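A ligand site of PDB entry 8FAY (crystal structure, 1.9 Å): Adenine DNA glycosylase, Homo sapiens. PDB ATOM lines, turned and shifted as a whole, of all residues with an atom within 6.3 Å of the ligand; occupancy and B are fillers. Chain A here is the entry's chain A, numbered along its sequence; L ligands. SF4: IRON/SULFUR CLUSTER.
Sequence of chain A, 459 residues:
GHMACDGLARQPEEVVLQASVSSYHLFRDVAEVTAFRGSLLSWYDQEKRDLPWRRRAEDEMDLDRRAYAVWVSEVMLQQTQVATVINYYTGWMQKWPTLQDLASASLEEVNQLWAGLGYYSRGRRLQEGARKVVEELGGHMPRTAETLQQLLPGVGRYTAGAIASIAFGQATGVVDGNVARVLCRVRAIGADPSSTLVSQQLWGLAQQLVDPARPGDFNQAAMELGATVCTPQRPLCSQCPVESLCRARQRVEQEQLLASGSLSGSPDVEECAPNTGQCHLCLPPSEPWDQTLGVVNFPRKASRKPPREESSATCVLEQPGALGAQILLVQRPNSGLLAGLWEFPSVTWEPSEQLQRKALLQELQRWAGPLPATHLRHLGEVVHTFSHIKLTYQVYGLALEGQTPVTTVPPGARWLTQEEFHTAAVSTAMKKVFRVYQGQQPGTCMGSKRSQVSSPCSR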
ATOM      1  N   ARG A 181       3.597  -1.888 -10.761  1.00  0.00           N
ATOM      2  CA  ARG A 181       4.233  -1.691  -9.462  1.00  0.00           C
ATOM      3  C   ARG A 181       5.686  -1.255  -9.625  1.00  0.00           C
ATOM      4  O   ARG A 181       6.128  -0.269  -9.023  1.00  0.00           O
ATOM      5  CB  ARG A 181       4.098  -2.975  -8.604  1.00  0.00           C
ATOM      6  CG  ARG A 181       4.922  -2.983  -7.276  1.00  0.00           C
ATOM      7  CD  ARG A 181       4.551  -4.180  -6.360  1.00  0.00           C
ATOM      8  NE  ARG A 181       4.743  -5.473  -7.024  1.00  0.00           N
ATOM      9  CZ  ARG A 181       3.773  -6.203  -7.549  1.00  0.00           C
ATOM     10  NH1 ARG A 181       2.505  -5.869  -7.433  1.00  0.00           N
ATOM     11  NH2 ARG A 181       4.090  -7.317  -8.216  1.00  0.00           N
ATOM     12  N   VAL A 182       6.451  -1.968 -10.448  1.00  0.00           N
ATOM     13  CA  VAL A 182       7.817  -1.563 -10.769  1.00  0.00           C
ATOM     14  C   VAL A 182       7.873  -0.118 -11.244  1.00  0.00           C
ATOM     15  O   VAL A 182       8.687   0.687 -10.767  1.00  0.00           O
ATOM     16  CB  VAL A 182       8.416  -2.512 -11.826  1.00  0.00           C
ATOM     17  CG1 VAL A 182       9.714  -1.942 -12.349  1.00  0.00           C
ATOM     18  CG2 VAL A 182       8.627  -3.933 -11.225  1.00  0.00           C
ATOM     19  N   ARG A 185       7.138   2.593  -8.697  1.00  0.00           N
ATOM     20  CA  ARG A 185       8.216   2.813  -7.736  1.00  0.00           C
ATOM     21  C   ARG A 185       9.411   3.484  -8.412  1.00  0.00           C
ATOM     22  O   ARG A 185       9.959   4.470  -7.906  1.00  0.00           O
ATOM     23  CB  ARG A 185       8.589   1.477  -7.053  1.00  0.00           C
ATOM     24  CG  ARG A 185       7.490   0.932  -6.126  1.00  0.00           C
ATOM     25  CD  ARG A 185       7.712  -0.510  -5.772  1.00  0.00           C
ATOM     26  NE  ARG A 185       6.732  -0.956  -4.802  1.00  0.00           N
ATOM     27  CZ  ARG A 185       6.689  -2.151  -4.246  1.00  0.00           C
ATOM     28  NH1 ARG A 185       7.604  -3.058  -4.509  1.00  0.00           N
ATOM     29  NH2 ARG A 185       5.704  -2.439  -3.409  1.00  0.00           N
ATOM     30  N   VAL A 186       9.808   2.998  -9.596  1.00  0.00           N
ATOM     31  CA  VAL A 186      10.952   3.571 -10.299  1.00  0.00           C
ATOM     32  C   VAL A 186      10.745   5.050 -10.585  1.00  0.00           C
ATOM     33  O   VAL A 186      11.695   5.835 -10.525  1.00  0.00           O
ATOM     34  CB  VAL A 186      11.229   2.791 -11.587  1.00  0.00           C
ATOM     35  CG1 VAL A 186      12.237   3.548 -12.444  1.00  0.00           C
ATOM     36  CG2 VAL A 186      11.738   1.397 -11.248  1.00  0.00           C
ATOM     37  N   LEU A 225      10.589  -9.254 -12.605  1.00  0.00           N
ATOM     38  CA  LEU A 225      11.111  -8.397 -11.552  1.00  0.00           C
ATOM     39  C   LEU A 225      10.019  -8.058 -10.574  1.00  0.00           C
ATOM     40  O   LEU A 225      10.207  -8.119  -9.361  1.00  0.00           O
ATOM     41  CB  LEU A 225      11.695  -7.120 -12.135  1.00  0.00           C
ATOM     42  CG  LEU A 225      12.323  -6.142 -11.150  1.00  0.00           C
ATOM     43  CD1 LEU A 225      13.637  -6.678 -10.770  1.00  0.00           C
ATOM     44  CD2 LEU A 225      12.470  -4.749 -11.717  1.00  0.00           C
ATOM     45  N   VAL A 229      11.280  -9.795  -7.200  1.00  0.00           N
ATOM     46  CA  VAL A 229      12.156  -8.824  -6.557  1.00  0.00           C
ATOM     47  C   VAL A 229      11.344  -7.642  -6.037  1.00  0.00           C
ATOM     48  O   VAL A 229      11.313  -7.393  -4.821  1.00  0.00           O
ATOM     49  CB  VAL A 229      13.249  -8.392  -7.531  1.00  0.00           C
ATOM     50  CG1 VAL A 229      14.072  -7.233  -6.984  1.00  0.00           C
ATOM     51  CG2 VAL A 229      14.162  -9.612  -7.860  1.00  0.00           C
ATOM     52  N   CYS A 230      10.691  -6.921  -6.949  1.00  0.00           N
ATOM     53  CA  CYS A 230       9.960  -5.701  -6.615  1.00  0.00           C
ATOM     54  C   CYS A 230       8.517  -6.097  -6.269  1.00  0.00           C
ATOM     55  O   CYS A 230       7.562  -5.825  -6.986  1.00  0.00           O
ATOM     56  CB  CYS A 230      10.027  -4.717  -7.774  1.00  0.00           C
ATOM     57  SG  CYS A 230       9.397  -3.063  -7.405  1.00  0.00           S
ATOM     58  N   THR A 231       8.406  -6.797  -5.145  1.00  0.00           N
ATOM     59  CA  THR A 231       7.175  -7.469  -4.774  1.00  0.00           C
ATOM     60  C   THR A 231       6.250  -6.528  -4.000  1.00  0.00           C
ATOM     61  O   THR A 231       6.646  -5.448  -3.535  1.00  0.00           O
ATOM     62  CB  THR A 231       7.518  -8.741  -3.977  1.00  0.00           C
ATOM     63  OG1 THR A 231       8.403  -8.448  -2.886  1.00  0.00           O
ATOM     64  CG2 THR A 231       8.254  -9.705  -4.899  1.00  0.00           C
ATOM     65  N   PRO A 235      10.061  -5.899  -0.763  1.00  0.00           N
ATOM     66  CA  PRO A 235      10.852  -5.937  -1.989  1.00  0.00           C
ATOM     67  C   PRO A 235      12.336  -6.039  -1.684  1.00  0.00           C
ATOM     68  O   PRO A 235      12.822  -5.558  -0.648  1.00  0.00           O
ATOM     69  CB  PRO A 235      10.507  -4.605  -2.681  1.00  0.00           C
ATOM     70  CG  PRO A 235      10.132  -3.718  -1.534  1.00  0.00           C
ATOM     71  CD  PRO A 235       9.436  -4.591  -0.556  1.00  0.00           C
ATOM     72  N   LEU A 236      13.050  -6.701  -2.583  1.00  0.00           N
ATOM     73  CA  LEU A 236      14.462  -7.002  -2.400  1.00  0.00           C
ATOM     74  C   LEU A 236      15.357  -5.967  -3.082  1.00  0.00           C
ATOM     75  O   LEU A 236      16.185  -6.305  -3.897  1.00  0.00           O
ATOM     76  CB  LEU A 236      14.752  -8.401  -2.923  1.00  0.00           C
ATOM     77  CG  LEU A 236      13.854  -9.492  -2.297  1.00  0.00           C
ATOM     78  CD1 LEU A 236      14.172 -10.870  -2.808  1.00  0.00           C
ATOM     79  CD2 LEU A 236      13.985  -9.493  -0.795  1.00  0.00           C
ATOM     80  N   CYS A 237      15.145  -4.684  -2.766  1.00  0.00           N
ATOM     81  CA  CYS A 237      15.845  -3.593  -3.448  1.00  0.00           C
ATOM     82  C   CYS A 237      17.346  -3.804  -3.509  1.00  0.00           C
ATOM     83  O   CYS A 237      17.991  -3.447  -4.503  1.00  0.00           O
ATOM     84  CB  CYS A 237      15.540  -2.265  -2.749  1.00  0.00           C
ATOM     85  SG  CYS A 237      13.777  -1.932  -2.562  1.00  0.00           S
ATOM     86  N   SER A 238      17.942  -4.364  -2.467  1.00  0.00           N
ATOM     87  CA  SER A 238      19.388  -4.524  -2.424  1.00  0.00           C
ATOM     88  C   SER A 238      19.910  -5.526  -3.437  1.00  0.00           C
ATOM     89  O   SER A 238      21.109  -5.497  -3.726  1.00  0.00           O
ATOM     90  CB  SER A 238      19.845  -4.971  -1.036  1.00  0.00           C
ATOM     91  OG  SER A 238      19.683  -3.875  -0.150  1.00  0.00           O
ATOM     92  N   CYS A 240      18.203  -5.744  -6.457  1.00  0.00           N
ATOM     93  CA  CYS A 240      17.414  -5.398  -7.627  1.00  0.00           C
ATOM     94  C   CYS A 240      18.325  -4.849  -8.747  1.00  0.00           C
ATOM     95  O   CYS A 240      19.158  -3.977  -8.494  1.00  0.00           O
ATOM     96  CB  CYS A 240      16.378  -4.360  -7.229  1.00  0.00           C
ATOM     97  SG  CYS A 240      15.423  -3.589  -8.597  1.00  0.00           S
ATOM     98  N   PRO A 241      18.177  -5.299  -9.988  1.00  0.00           N
ATOM     99  CA  PRO A 241      19.057  -4.805 -11.056  1.00  0.00           C
ATOM    100  C   PRO A 241      18.899  -3.333 -11.381  1.00  0.00           C
ATOM    101  O   PRO A 241      19.839  -2.769 -11.964  1.00  0.00           O
ATOM    102  CB  PRO A 241      18.671  -5.667 -12.273  1.00  0.00           C
ATOM    103  CG  PRO A 241      17.251  -6.092 -11.979  1.00  0.00           C
ATOM    104  CD  PRO A 241      17.147  -6.226 -10.502  1.00  0.00           C
ATOM    105  N   VAL A 242      17.791  -2.683 -11.040  1.00  0.00           N
ATOM    106  CA  VAL A 242      17.554  -1.303 -11.449  1.00  0.00           C
ATOM    107  C   VAL A 242      17.559  -0.343 -10.264  1.00  0.00           C
ATOM    108  O   VAL A 242      17.134   0.791 -10.423  1.00  0.00           O
ATOM    109  CB  VAL A 242      16.270  -1.149 -12.293  1.00  0.00           C
ATOM    110  CG1 VAL A 242      16.442  -1.890 -13.591  1.00  0.00           C
ATOM    111  CG2 VAL A 242      15.012  -1.612 -11.522  1.00  0.00           C
ATOM    112  N   GLU A 243      18.100  -0.780  -9.108  1.00  0.00           N
ATOM    113  CA  GLU A 243      18.092  -0.011  -7.867  1.00  0.00           C
ATOM    114  C   GLU A 243      18.610   1.430  -8.023  1.00  0.00           C
ATOM    115  O   GLU A 243      18.058   2.377  -7.440  1.00  0.00           O
ATOM    116  CB  GLU A 243      18.945  -0.799  -6.837  1.00  0.00           C
ATOM    117  CG  GLU A 243      19.287  -0.049  -5.555  1.00  0.00           C
ATOM    118  CD  GLU A 243      20.205  -0.829  -4.618  1.00  0.00           C
ATOM    119  OE1 GLU A 243      20.833  -1.826  -5.053  1.00  0.00           O
ATOM    120  OE2 GLU A 243      20.306  -0.410  -3.445  1.00  0.00           O
ATOM    121  N   SER A 244      19.705   1.608  -8.747  1.00  0.00           N
ATOM    122  CA  SER A 244      20.302   2.937  -8.884  1.00  0.00           C
ATOM    123  C   SER A 244      19.476   3.865  -9.749  1.00  0.00           C
ATOM    124  O   SER A 244      19.688   5.071  -9.696  1.00  0.00           O
ATOM    125  CB  SER A 244      21.700   2.828  -9.490  1.00  0.00           C
ATOM    126  OG  SER A 244      21.559   2.471 -10.840  1.00  0.00           O
ATOM    127  N   CYS A 246      16.037   3.725  -9.544  1.00  0.00           N
ATOM    128  CA  CYS A 246      14.697   3.728  -8.954  1.00  0.00           C
ATOM    129  C   CYS A 246      14.486   4.941  -8.027  1.00  0.00           C
ATOM    130  O   CYS A 246      15.155   5.064  -6.993  1.00  0.00           O
ATOM    131  CB  CYS A 246      14.473   2.426  -8.169  1.00  0.00           C
ATOM    132  SG  CYS A 246      12.920   2.449  -7.231  1.00  0.00           S
ATOM    133  N   ARG A 247      13.510   5.781  -8.349  1.00  0.00           N
ATOM    134  CA  ARG A 247      13.312   6.966  -7.505  1.00  0.00           C
ATOM    135  C   ARG A 247      12.844   6.627  -6.104  1.00  0.00           C
ATOM    136  O   ARG A 247      13.182   7.332  -5.143  1.00  0.00           O
ATOM    137  CB  ARG A 247      12.336   7.940  -8.162  1.00  0.00           C
ATOM    138  CG  ARG A 247      13.086   8.932  -9.081  1.00  0.00           C
ATOM    139  CD  ARG A 247      12.134   9.707  -9.955  1.00  0.00           C
ATOM    140  NE  ARG A 247      12.845  10.403 -11.023  1.00  0.00           N
ATOM    141  CZ  ARG A 247      12.254  11.087 -11.992  1.00  0.00           C
ATOM    142  NH1 ARG A 247      10.929  11.248 -12.024  1.00  0.00           N
ATOM    143  NH2 ARG A 247      13.002  11.628 -12.958  1.00  0.00           N
ATOM    144  N   ALA A 248      11.995   5.618  -5.939  1.00  0.00           N
ATOM    145  CA  ALA A 248      11.518   5.342  -4.587  1.00  0.00           C
ATOM    146  C   ALA A 248      12.670   4.871  -3.718  1.00  0.00           C
ATOM    147  O   ALA A 248      12.836   5.336  -2.588  1.00  0.00           O
ATOM    148  CB  ALA A 248      10.380   4.330  -4.624  1.00  0.00           C
ATOM    149  N   ARG A 249      13.513   3.990  -4.276  1.00  0.00           N
ATOM    150  CA  ARG A 249      14.687   3.506  -3.564  1.00  0.00           C
ATOM    151  C   ARG A 249      15.606   4.656  -3.172  1.00  0.00           C
ATOM    152  O   ARG A 249      16.151   4.670  -2.060  1.00  0.00           O
ATOM    153  CB  ARG A 249      15.440   2.517  -4.457  1.00  0.00           C
ATOM    154  CG  ARG A 249      16.712   1.985  -3.884  1.00  0.00           C
ATOM    155  CD  ARG A 249      16.489   1.228  -2.563  1.00  0.00           C
ATOM    156  NE  ARG A 249      17.684   0.504  -2.162  1.00  0.00           N
ATOM    157  CZ  ARG A 249      17.835  -0.127  -1.003  1.00  0.00           C
ATOM    158  NH1 ARG A 249      16.879  -0.129  -0.074  1.00  0.00           N
ATOM    159  NH2 ARG A 249      18.965  -0.767  -0.762  1.00  0.00           N
ATOM    160  N   VAL A 295       9.428   2.086  -0.085  1.00  0.00           N
ATOM    161  CA  VAL A 295       9.030   2.058  -1.491  1.00  0.00           C
ATOM    162  C   VAL A 295       7.620   1.498  -1.640  1.00  0.00           C
ATOM    163  O   VAL A 295       6.946   1.700  -2.668  1.00  0.00           O
ATOM    164  CB  VAL A 295      10.051   1.265  -2.341  1.00  0.00           C
ATOM    165  CG1 VAL A 295      11.487   1.788  -2.136  1.00  0.00           C
ATOM    166  CG2 VAL A 295       9.980  -0.215  -2.000  1.00  0.00           C
HETATM  167 FE1  SF4 L   1      14.020  -2.315  -7.423  1.00  0.00          FE
HETATM  168 FE2  SF4 L   1      11.351  -2.098  -6.797  1.00  0.00          FE
HETATM  169 FE3  SF4 L   1      12.972   0.096  -6.871  1.00  0.00          FE
HETATM  170 FE4  SF4 L   1      13.190  -1.714  -4.821  1.00  0.00          FE
HETATM  171  S1  SF4 L   1      11.342  -0.431  -5.305  1.00  0.00           S
HETATM  172  S2  SF4 L   1      14.906  -0.745  -6.043  1.00  0.00           S
HETATM  173  S3  SF4 L   1      12.816  -3.650  -5.906  1.00  0.00           S
HETATM  174  S4  SF4 L   1      12.479  -1.244  -8.679  1.00  0.00           S
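FE3 of the ligand is bound by SG of Cys 246 (2.4 Å).
FE2 of the ligand is bound by SG of Cys 230 (2.3 Å).
The side-chain sulfur (SG) of Cys 237 is bound to an iron atom (FE4) of the ligand (2.3 Å).
The side-chain sulfur (SG) of Cys 240 binds an iron atom (FE1) of the ligand.
The guanidinium group of Arg 185 lies close to the side-chain sulfur of Cys 230 (3.4 Å).
The backbone carbonyl oxygen of Cys 230 sits at hydrogen-bond distance from the guanidinium group of Arg 181.
The side-chain sulfur (SG) of Cys 246 sits close to the backbone carbonyl oxygen (O) of Arg 185 (3.6 Å).
The side-chain carboxylate (OE2) of Glu 243 is in salt-bridge range of the guanidinium group (NH2) of Arg 249.
N of Leu 236 lies within hydrogen-bond range of O of Val 229 (2.9 Å).
N of Ala 248 is in hydrogen-bond range of O of Arg 185, 3.1 Å away.
The backbone NH of Cys 230 sits at hydrogen-bond distance from the backbone carbonyl oxygen of Leu 225 (2.7 Å).
The side-chain sulfur of Cys 246 lies close to the backbone NH of Ala 248 (3.5 Å).
CD of Arg 185 touches S1 of the ligand, at 3.7 Å.
Val 186 touches the ligand (CG2 to S4, 3.8 Å).
CG1 of Val 229 touches S3 of the ligand, at 3.9 Å.
CG2 of Val 242 touches S4 of the ligand, 3.8 Å away.
Glu 243 touches the ligand (CA to S2, 3.7 Å).
Arg 249 touches the ligand (CB to S2, 3.7 Å).
Val 295 touches the ligand.
Of the 22 residues printed, 11 come within 4 Å of the ligand.
Along chain A the residues within 4 Å of the ligand span positions 185 to 295.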
